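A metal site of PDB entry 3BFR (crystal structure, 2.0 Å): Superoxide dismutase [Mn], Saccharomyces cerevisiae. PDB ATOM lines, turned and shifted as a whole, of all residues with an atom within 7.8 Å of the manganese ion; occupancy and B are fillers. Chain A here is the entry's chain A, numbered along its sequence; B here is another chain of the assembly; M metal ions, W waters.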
ATOM      1  N   HIS A  34      28.872  11.369 -15.839  1.00  0.00           N
ATOM      2  CA  HIS A  34      28.320  11.595 -14.503  1.00  0.00           C
ATOM      3  C   HIS A  34      27.686  10.320 -13.910  1.00  0.00           C
ATOM      4  O   HIS A  34      27.841  10.019 -12.712  1.00  0.00           O
ATOM      5  CB  HIS A  34      27.263  12.685 -14.594  1.00  0.00           C
ATOM      6  CG  HIS A  34      27.083  13.491 -13.342  1.00  0.00           C
ATOM      7  ND1 HIS A  34      26.288  14.615 -13.300  1.00  0.00           N
ATOM      8  CD2 HIS A  34      27.605  13.334 -12.107  1.00  0.00           C
ATOM      9  CE1 HIS A  34      26.319  15.114 -12.083  1.00  0.00           C
ATOM     10  NE2 HIS A  34      27.109  14.367 -11.330  1.00  0.00           N
ATOM     11  N   TYR A  35      26.978   9.578 -14.752  1.00  0.00           N
ATOM     12  CA  TYR A  35      26.310   8.338 -14.384  1.00  0.00           C
ATOM     13  C   TYR A  35      27.244   7.117 -14.406  1.00  0.00           C
ATOM     14  O   TYR A  35      27.411   6.438 -13.390  1.00  0.00           O
ATOM     15  CB  TYR A  35      25.102   8.126 -15.315  1.00  0.00           C
ATOM     16  CG  TYR A  35      24.301   6.871 -15.088  1.00  0.00           C
ATOM     17  CD1 TYR A  35      23.308   6.815 -14.110  1.00  0.00           C
ATOM     18  CD2 TYR A  35      24.495   5.749 -15.894  1.00  0.00           C
ATOM     19  CE1 TYR A  35      22.548   5.670 -13.921  1.00  0.00           C
ATOM     20  CE2 TYR A  35      23.743   4.591 -15.714  1.00  0.00           C
ATOM     21  CZ  TYR A  35      22.766   4.563 -14.728  1.00  0.00           C
ATOM     22  OH  TYR A  35      22.026   3.412 -14.548  1.00  0.00           O
ATOM     23  N   HIS A  38      31.251   8.691 -12.507  1.00  0.00           N
ATOM     24  CA  HIS A  38      31.175   9.350 -11.193  1.00  0.00           C
ATOM     25  C   HIS A  38      30.236   8.626 -10.226  1.00  0.00           C
ATOM     26  O   HIS A  38      30.637   8.265  -9.118  1.00  0.00           O
ATOM     27  CB  HIS A  38      30.793  10.838 -11.350  1.00  0.00           C
ATOM     28  CG  HIS A  38      31.837  11.644 -12.070  1.00  0.00           C
ATOM     29  ND1 HIS A  38      32.991  12.077 -11.458  1.00  0.00           N
ATOM     30  CD2 HIS A  38      31.907  12.077 -13.354  1.00  0.00           C
ATOM     31  CE1 HIS A  38      33.726  12.747 -12.325  1.00  0.00           C
ATOM     32  NE2 HIS A  38      33.093  12.761 -13.492  1.00  0.00           N
ATOM     33  N   HIS A  39      28.993   8.396 -10.645  1.00  0.00           N
ATOM     34  CA  HIS A  39      28.017   7.716  -9.791  1.00  0.00           C
ATOM     35  C   HIS A  39      28.459   6.286  -9.447  1.00  0.00           C
ATOM     36  O   HIS A  39      28.378   5.869  -8.285  1.00  0.00           O
ATOM     37  CB  HIS A  39      26.623   7.707 -10.430  1.00  0.00           C
ATOM     38  CG  HIS A  39      25.498   7.541  -9.457  1.00  0.00           C
ATOM     39  ND1 HIS A  39      25.703   7.299  -8.112  1.00  0.00           N
ATOM     40  CD2 HIS A  39      24.160   7.580  -9.627  1.00  0.00           C
ATOM     41  CE1 HIS A  39      24.535   7.191  -7.505  1.00  0.00           C
ATOM     42  NE2 HIS A  39      23.580   7.361  -8.399  1.00  0.00           N
ATOM     43  N   TYR A  42      31.045   6.108  -6.655  1.00  0.00           N
ATOM     44  CA  TYR A  42      30.441   6.213  -5.321  1.00  0.00           C
ATOM     45  C   TYR A  42      29.746   4.909  -4.928  1.00  0.00           C
ATOM     46  O   TYR A  42      29.836   4.477  -3.772  1.00  0.00           O
ATOM     47  CB  TYR A  42      29.488   7.412  -5.237  1.00  0.00           C
ATOM     48  CG  TYR A  42      30.155   8.741  -5.512  1.00  0.00           C
ATOM     49  CD1 TYR A  42      31.260   9.165  -4.759  1.00  0.00           C
ATOM     50  CD2 TYR A  42      29.682   9.595  -6.517  1.00  0.00           C
ATOM     51  CE1 TYR A  42      31.886  10.382  -5.007  1.00  0.00           C
ATOM     52  CE2 TYR A  42      30.299  10.814  -6.775  1.00  0.00           C
ATOM     53  CZ  TYR A  42      31.394  11.199  -6.019  1.00  0.00           C
ATOM     54  OH  TYR A  42      31.998  12.412  -6.267  1.00  0.00           O
ATOM     55  N   GLY A  85      27.675  10.352  -1.928  1.00  0.00           N
ATOM     56  CA  GLY A  85      27.767  10.332  -3.389  1.00  0.00           C
ATOM     57  C   GLY A  85      26.717   9.455  -4.038  1.00  0.00           C
ATOM     58  O   GLY A  85      26.110   9.836  -5.050  1.00  0.00           O
ATOM     59  N   ASN A  88      23.047  11.231  -3.077  1.00  0.00           N
ATOM     60  CA  ASN A  88      22.862  12.530  -3.738  1.00  0.00           C
ATOM     61  C   ASN A  88      22.588  12.408  -5.218  1.00  0.00           C
ATOM     62  O   ASN A  88      21.728  13.117  -5.738  1.00  0.00           O
ATOM     63  CB  ASN A  88      24.068  13.463  -3.501  1.00  0.00           C
ATOM     64  CG  ASN A  88      24.117  14.022  -2.097  1.00  0.00           C
ATOM     65  OD1 ASN A  88      23.108  14.026  -1.375  1.00  0.00           O
ATOM     66  ND2 ASN A  88      25.291  14.498  -1.688  1.00  0.00           N
ATOM     67  N   HIS A  89      23.304  11.520  -5.911  1.00  0.00           N
ATOM     68  CA  HIS A  89      23.114  11.368  -7.358  1.00  0.00           C
ATOM     69  C   HIS A  89      21.801  10.643  -7.692  1.00  0.00           C
ATOM     70  O   HIS A  89      21.182  10.934  -8.708  1.00  0.00           O
ATOM     71  CB  HIS A  89      24.319  10.695  -8.017  1.00  0.00           C
ATOM     72  CG  HIS A  89      25.532  11.575  -8.058  1.00  0.00           C
ATOM     73  ND1 HIS A  89      26.404  11.667  -7.004  1.00  0.00           N
ATOM     74  CD2 HIS A  89      25.994  12.415  -9.013  1.00  0.00           C
ATOM     75  CE1 HIS A  89      27.365  12.534  -7.300  1.00  0.00           C
ATOM     76  NE2 HIS A  89      27.130  13.000  -8.512  1.00  0.00           N
ATOM     77  N   PHE A  92      19.390  13.292  -7.472  1.00  0.00           N
ATOM     78  CA  PHE A  92      19.638  14.153  -8.624  1.00  0.00           C
ATOM     79  C   PHE A  92      18.912  13.677  -9.897  1.00  0.00           C
ATOM     80  O   PHE A  92      18.143  14.452 -10.470  1.00  0.00           O
ATOM     81  CB  PHE A  92      21.154  14.297  -8.875  1.00  0.00           C
ATOM     82  CG  PHE A  92      21.527  15.386  -9.860  1.00  0.00           C
ATOM     83  CD1 PHE A  92      21.095  16.694  -9.674  1.00  0.00           C
ATOM     84  CD2 PHE A  92      22.351  15.095 -10.946  1.00  0.00           C
ATOM     85  CE1 PHE A  92      21.446  17.710 -10.584  1.00  0.00           C
ATOM     86  CE2 PHE A  92      22.707  16.090 -11.854  1.00  0.00           C
ATOM     87  CZ  PHE A  92      22.256  17.402 -11.679  1.00  0.00           C
ATOM     88  N   TRP A  93      19.131  12.431 -10.312  1.00  0.00           N
ATOM     89  CA  TRP A  93      18.491  11.894 -11.529  1.00  0.00           C
ATOM     90  C   TRP A  93      16.965  11.889 -11.408  1.00  0.00           C
ATOM     91  O   TRP A  93      16.262  12.185 -12.367  1.00  0.00           O
ATOM     92  CB  TRP A  93      18.951  10.476 -11.867  1.00  0.00           C
ATOM     93  CG  TRP A  93      20.433  10.255 -11.822  1.00  0.00           C
ATOM     94  CD1 TRP A  93      21.091   9.268 -11.145  1.00  0.00           C
ATOM     95  CD2 TRP A  93      21.435  11.024 -12.490  1.00  0.00           C
ATOM     96  NE1 TRP A  93      22.442   9.387 -11.338  1.00  0.00           N
ATOM     97  CE2 TRP A  93      22.688  10.448 -12.153  1.00  0.00           C
ATOM     98  CE3 TRP A  93      21.407  12.144 -13.335  1.00  0.00           C
ATOM     99  CZ2 TRP A  93      23.897  10.967 -12.638  1.00  0.00           C
ATOM    100  CZ3 TRP A  93      22.623  12.652 -13.810  1.00  0.00           C
ATOM    101  CH2 TRP A  93      23.849  12.054 -13.451  1.00  0.00           C
ATOM    102  N   GLY A 140      30.216  20.817  -4.160  1.00  0.00           N
ATOM    103  CA  GLY A 140      29.079  20.595  -3.274  1.00  0.00           C
ATOM    104  C   GLY A 140      27.727  20.583  -3.952  1.00  0.00           C
ATOM    105  O   GLY A 140      27.621  20.353  -5.160  1.00  0.00           O
ATOM    106  N   TRP A 141      26.699  20.846  -3.149  1.00  0.00           N
ATOM    107  CA  TRP A 141      25.309  20.727  -3.569  1.00  0.00           C
ATOM    108  C   TRP A 141      24.489  21.873  -2.997  1.00  0.00           C
ATOM    109  O   TRP A 141      24.872  22.462  -1.990  1.00  0.00           O
ATOM    110  CB  TRP A 141      24.718  19.405  -3.052  1.00  0.00           C
ATOM    111  CG  TRP A 141      25.334  18.186  -3.652  1.00  0.00           C
ATOM    112  CD1 TRP A 141      26.512  17.599  -3.315  1.00  0.00           C
ATOM    113  CD2 TRP A 141      24.782  17.379  -4.707  1.00  0.00           C
ATOM    114  NE1 TRP A 141      26.750  16.489  -4.092  1.00  0.00           N
ATOM    115  CE2 TRP A 141      25.699  16.333  -4.963  1.00  0.00           C
ATOM    116  CE3 TRP A 141      23.597  17.442  -5.457  1.00  0.00           C
ATOM    117  CZ2 TRP A 141      25.473  15.362  -5.940  1.00  0.00           C
ATOM    118  CZ3 TRP A 141      23.372  16.471  -6.434  1.00  0.00           C
ATOM    119  CH2 TRP A 141      24.303  15.444  -6.661  1.00  0.00           C
ATOM    120  N   ASN A 161      31.104  18.924  -0.835  1.00  0.00           N
ATOM    121  CA  ASN A 161      31.603  17.605  -1.230  1.00  0.00           C
ATOM    122  C   ASN A 161      30.420  16.675  -1.496  1.00  0.00           C
ATOM    123  O   ASN A 161      29.574  16.997  -2.318  1.00  0.00           O
ATOM    124  CB  ASN A 161      32.598  17.093  -0.190  1.00  0.00           C
ATOM    125  CG  ASN A 161      33.706  18.096   0.089  1.00  0.00           C
ATOM    126  OD1 ASN A 161      34.013  18.415   1.245  1.00  0.00           O
ATOM    127  ND2 ASN A 161      34.299  18.624  -0.971  1.00  0.00           N
ATOM    128  N   GLN A 162      30.355  15.538  -0.792  1.00  0.00           N
ATOM    129  CA  GLN A 162      29.172  14.672  -0.882  1.00  0.00           C
ATOM    130  C   GLN A 162      28.371  14.608   0.411  1.00  0.00           C
ATOM    131  O   GLN A 162      27.652  13.634   0.669  1.00  0.00           O
ATOM    132  CB  GLN A 162      29.534  13.248  -1.372  1.00  0.00           C
ATOM    133  CG  GLN A 162      30.115  13.166  -2.779  1.00  0.00           C
ATOM    134  CD  GLN A 162      29.192  13.708  -3.860  1.00  0.00           C
ATOM    135  OE1 GLN A 162      28.010  13.972  -3.632  1.00  0.00           O
ATOM    136  NE2 GLN A 162      29.730  13.889  -5.056  1.00  0.00           N
ATOM    137  N   ASP A 176      23.419  19.470  -8.317  1.00  0.00           N
ATOM    138  CA  ASP A 176      24.851  19.181  -8.248  1.00  0.00           C
ATOM    139  C   ASP A 176      25.650  20.404  -8.663  1.00  0.00           C
ATOM    140  O   ASP A 176      25.457  20.929  -9.758  1.00  0.00           O
ATOM    141  CB  ASP A 176      25.165  17.990  -9.157  1.00  0.00           C
ATOM    142  CG  ASP A 176      26.506  17.348  -8.843  1.00  0.00           C
ATOM    143  OD1 ASP A 176      26.804  16.295  -9.462  1.00  0.00           O
ATOM    144  OD2 ASP A 176      27.258  17.861  -7.993  1.00  0.00           O
ATOM    145  N   ALA A 177      26.552  20.859  -7.786  1.00  0.00           N
ATOM    146  CA  ALA A 177      27.447  21.993  -8.062  1.00  0.00           C
ATOM    147  C   ALA A 177      28.919  21.583  -8.254  1.00  0.00           C
ATOM    148  O   ALA A 177      29.780  22.444  -8.410  1.00  0.00           O
ATOM    149  CB  ALA A 177      27.319  23.056  -6.959  1.00  0.00           C
ATOM    150  N   TRP A 178      29.199  20.279  -8.213  1.00  0.00           N
ATOM    151  CA  TRP A 178      30.531  19.780  -8.571  1.00  0.00           C
ATOM    152  C   TRP A 178      30.831  20.205 -10.000  1.00  0.00           C
ATOM    153  O   TRP A 178      29.941  20.194 -10.860  1.00  0.00           O
ATOM    154  CB  TRP A 178      30.596  18.257  -8.468  1.00  0.00           C
ATOM    155  CG  TRP A 178      30.763  17.718  -7.071  1.00  0.00           C
ATOM    156  CD1 TRP A 178      29.894  17.873  -6.017  1.00  0.00           C
ATOM    157  CD2 TRP A 178      31.849  16.917  -6.580  1.00  0.00           C
ATOM    158  NE1 TRP A 178      30.374  17.222  -4.907  1.00  0.00           N
ATOM    159  CE2 TRP A 178      31.566  16.628  -5.221  1.00  0.00           C
ATOM    160  CE3 TRP A 178      33.022  16.414  -7.152  1.00  0.00           C
ATOM    161  CZ2 TRP A 178      32.442  15.861  -4.425  1.00  0.00           C
ATOM    162  CZ3 TRP A 178      33.889  15.650  -6.357  1.00  0.00           C
ATOM    163  CH2 TRP A 178      33.592  15.384  -5.019  1.00  0.00           C
ATOM    164  N   GLU A 179      32.077  20.585 -10.254  1.00  0.00           N
ATOM    165  CA  GLU A 179      32.478  21.011 -11.592  1.00  0.00           C
ATOM    166  C   GLU A 179      32.203  19.952 -12.673  1.00  0.00           C
ATOM    167  O   GLU A 179      31.863  20.307 -13.799  1.00  0.00           O
ATOM    168  CB  GLU A 179      33.929  21.499 -11.599  1.00  0.00           C
ATOM    169  CG  GLU A 179      34.110  22.791 -10.797  1.00  0.00           C
ATOM    170  CD  GLU A 179      35.543  23.296 -10.786  1.00  0.00           C
ATOM    171  OE1 GLU A 179      36.461  22.492 -10.519  1.00  0.00           O
ATOM    172  OE2 GLU A 179      35.752  24.498 -11.041  1.00  0.00           O
ATOM    173  N   HIS A 180      32.321  18.670 -12.326  1.00  0.00           N
ATOM    174  CA  HIS A 180      32.036  17.591 -13.295  1.00  0.00           C
ATOM    175  C   HIS A 180      30.579  17.598 -13.796  1.00  0.00           C
ATOM    176  O   HIS A 180      30.264  16.988 -14.830  1.00  0.00           O
ATOM    177  CB  HIS A 180      32.443  16.214 -12.765  1.00  0.00           C
ATOM    178  CG  HIS A 180      31.617  15.713 -11.611  1.00  0.00           C
ATOM    179  ND1 HIS A 180      32.166  15.382 -10.393  1.00  0.00           N
ATOM    180  CD2 HIS A 180      30.295  15.456 -11.508  1.00  0.00           C
ATOM    181  CE1 HIS A 180      31.218  14.961  -9.578  1.00  0.00           C
ATOM    182  NE2 HIS A 180      30.063  14.992 -10.235  1.00  0.00           N
ATOM    183  N   ALA A 181      29.710  18.301 -13.072  1.00  0.00           N
ATOM    184  CA  ALA A 181      28.289  18.391 -13.427  1.00  0.00           C
ATOM    185  C   ALA A 181      28.039  19.319 -14.604  1.00  0.00           C
ATOM    186  O   ALA A 181      26.964  19.270 -15.213  1.00  0.00           O
ATOM    187  CB  ALA A 181      27.466  18.824 -12.222  1.00  0.00           C
ATOM    188  N   TYR A 193      25.007  27.349 -16.125  1.00  0.00           N
ATOM    189  CA  TYR A 193      24.514  26.019 -15.806  1.00  0.00           C
ATOM    190  C   TYR A 193      23.401  26.072 -14.759  1.00  0.00           C
ATOM    191  O   TYR A 193      22.356  25.443 -14.944  1.00  0.00           O
ATOM    192  CB  TYR A 193      25.672  25.133 -15.358  1.00  0.00           C
ATOM    193  CG  TYR A 193      25.280  23.902 -14.563  1.00  0.00           C
ATOM    194  CD1 TYR A 193      24.612  22.834 -15.170  1.00  0.00           C
ATOM    195  CD2 TYR A 193      25.603  23.796 -13.205  1.00  0.00           C
ATOM    196  CE1 TYR A 193      24.268  21.700 -14.441  1.00  0.00           C
ATOM    197  CE2 TYR A 193      25.251  22.674 -12.468  1.00  0.00           C
ATOM    198  CZ  TYR A 193      24.586  21.615 -13.095  1.00  0.00           C
ATOM    199  OH  TYR A 193      24.238  20.502 -12.368  1.00  0.00           O
ATOM    200  N   GLU B 179      38.610  19.731 -10.063  1.00  0.00           N
ATOM    201  CA  GLU B 179      38.261  19.114 -11.339  1.00  0.00           C
ATOM    202  C   GLU B 179      38.581  20.004 -12.551  1.00  0.00           C
ATOM    203  O   GLU B 179      38.964  19.490 -13.599  1.00  0.00           O
ATOM    204  CB  GLU B 179      36.810  18.625 -11.331  1.00  0.00           C
ATOM    205  CG  GLU B 179      36.594  17.463 -10.358  1.00  0.00           C
ATOM    206  CD  GLU B 179      35.160  16.962 -10.329  1.00  0.00           C
ATOM    207  OE1 GLU B 179      34.234  17.793 -10.218  1.00  0.00           O
ATOM    208  OE2 GLU B 179      34.957  15.735 -10.414  1.00  0.00           O
HETATM  209 MN    MN M   1      28.064  14.762  -9.315  1.00  0.00          MN
HETATM  210  O   HOH W   1      28.755  15.437  -7.385  1.00  0.00           O
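OD2 of Asp 176 lies within hydrogen-bond range of N of Trp 178, 3.1 Å away. O of Asp 176 is in hydrogen-bond range of OH of Tyr 193 (2.9 Å). O of His 89 sits close to NE1 of Trp 93 (3.3 Å). A ring nitrogen (ND1) of His 89 is in hydrogen-bond range of the backbone carbonyl oxygen (O) of Gly 85. The side-chain carboxylate of Glu 179 of chain B sits at hydrogen-bond distance from a ring nitrogen (ND1) of His 180 (2.8 Å). The backbone carbonyl oxygen of His 34 sits at hydrogen-bond distance from the backbone NH of His 39 (2.9 Å).
Within 4 Å of the manganese ion: His 34, His 89, Asp 176 and His 180.
The manganese ion is bound by OD1 of Asp 176 (2.0 Å), NE2 of His 89 (2.1 Å), water W1 (2.2 Å), NE2 of His 180 (2.2 Å) and NE2 of His 34 (2.3 Å).
Water W1 lies within hydrogen-bond range of OD2 of Asp 176 (2.9 Å), NE2 of Gln 162 (3.0 Å) and NE1 of Trp 178 (3.5 Å).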
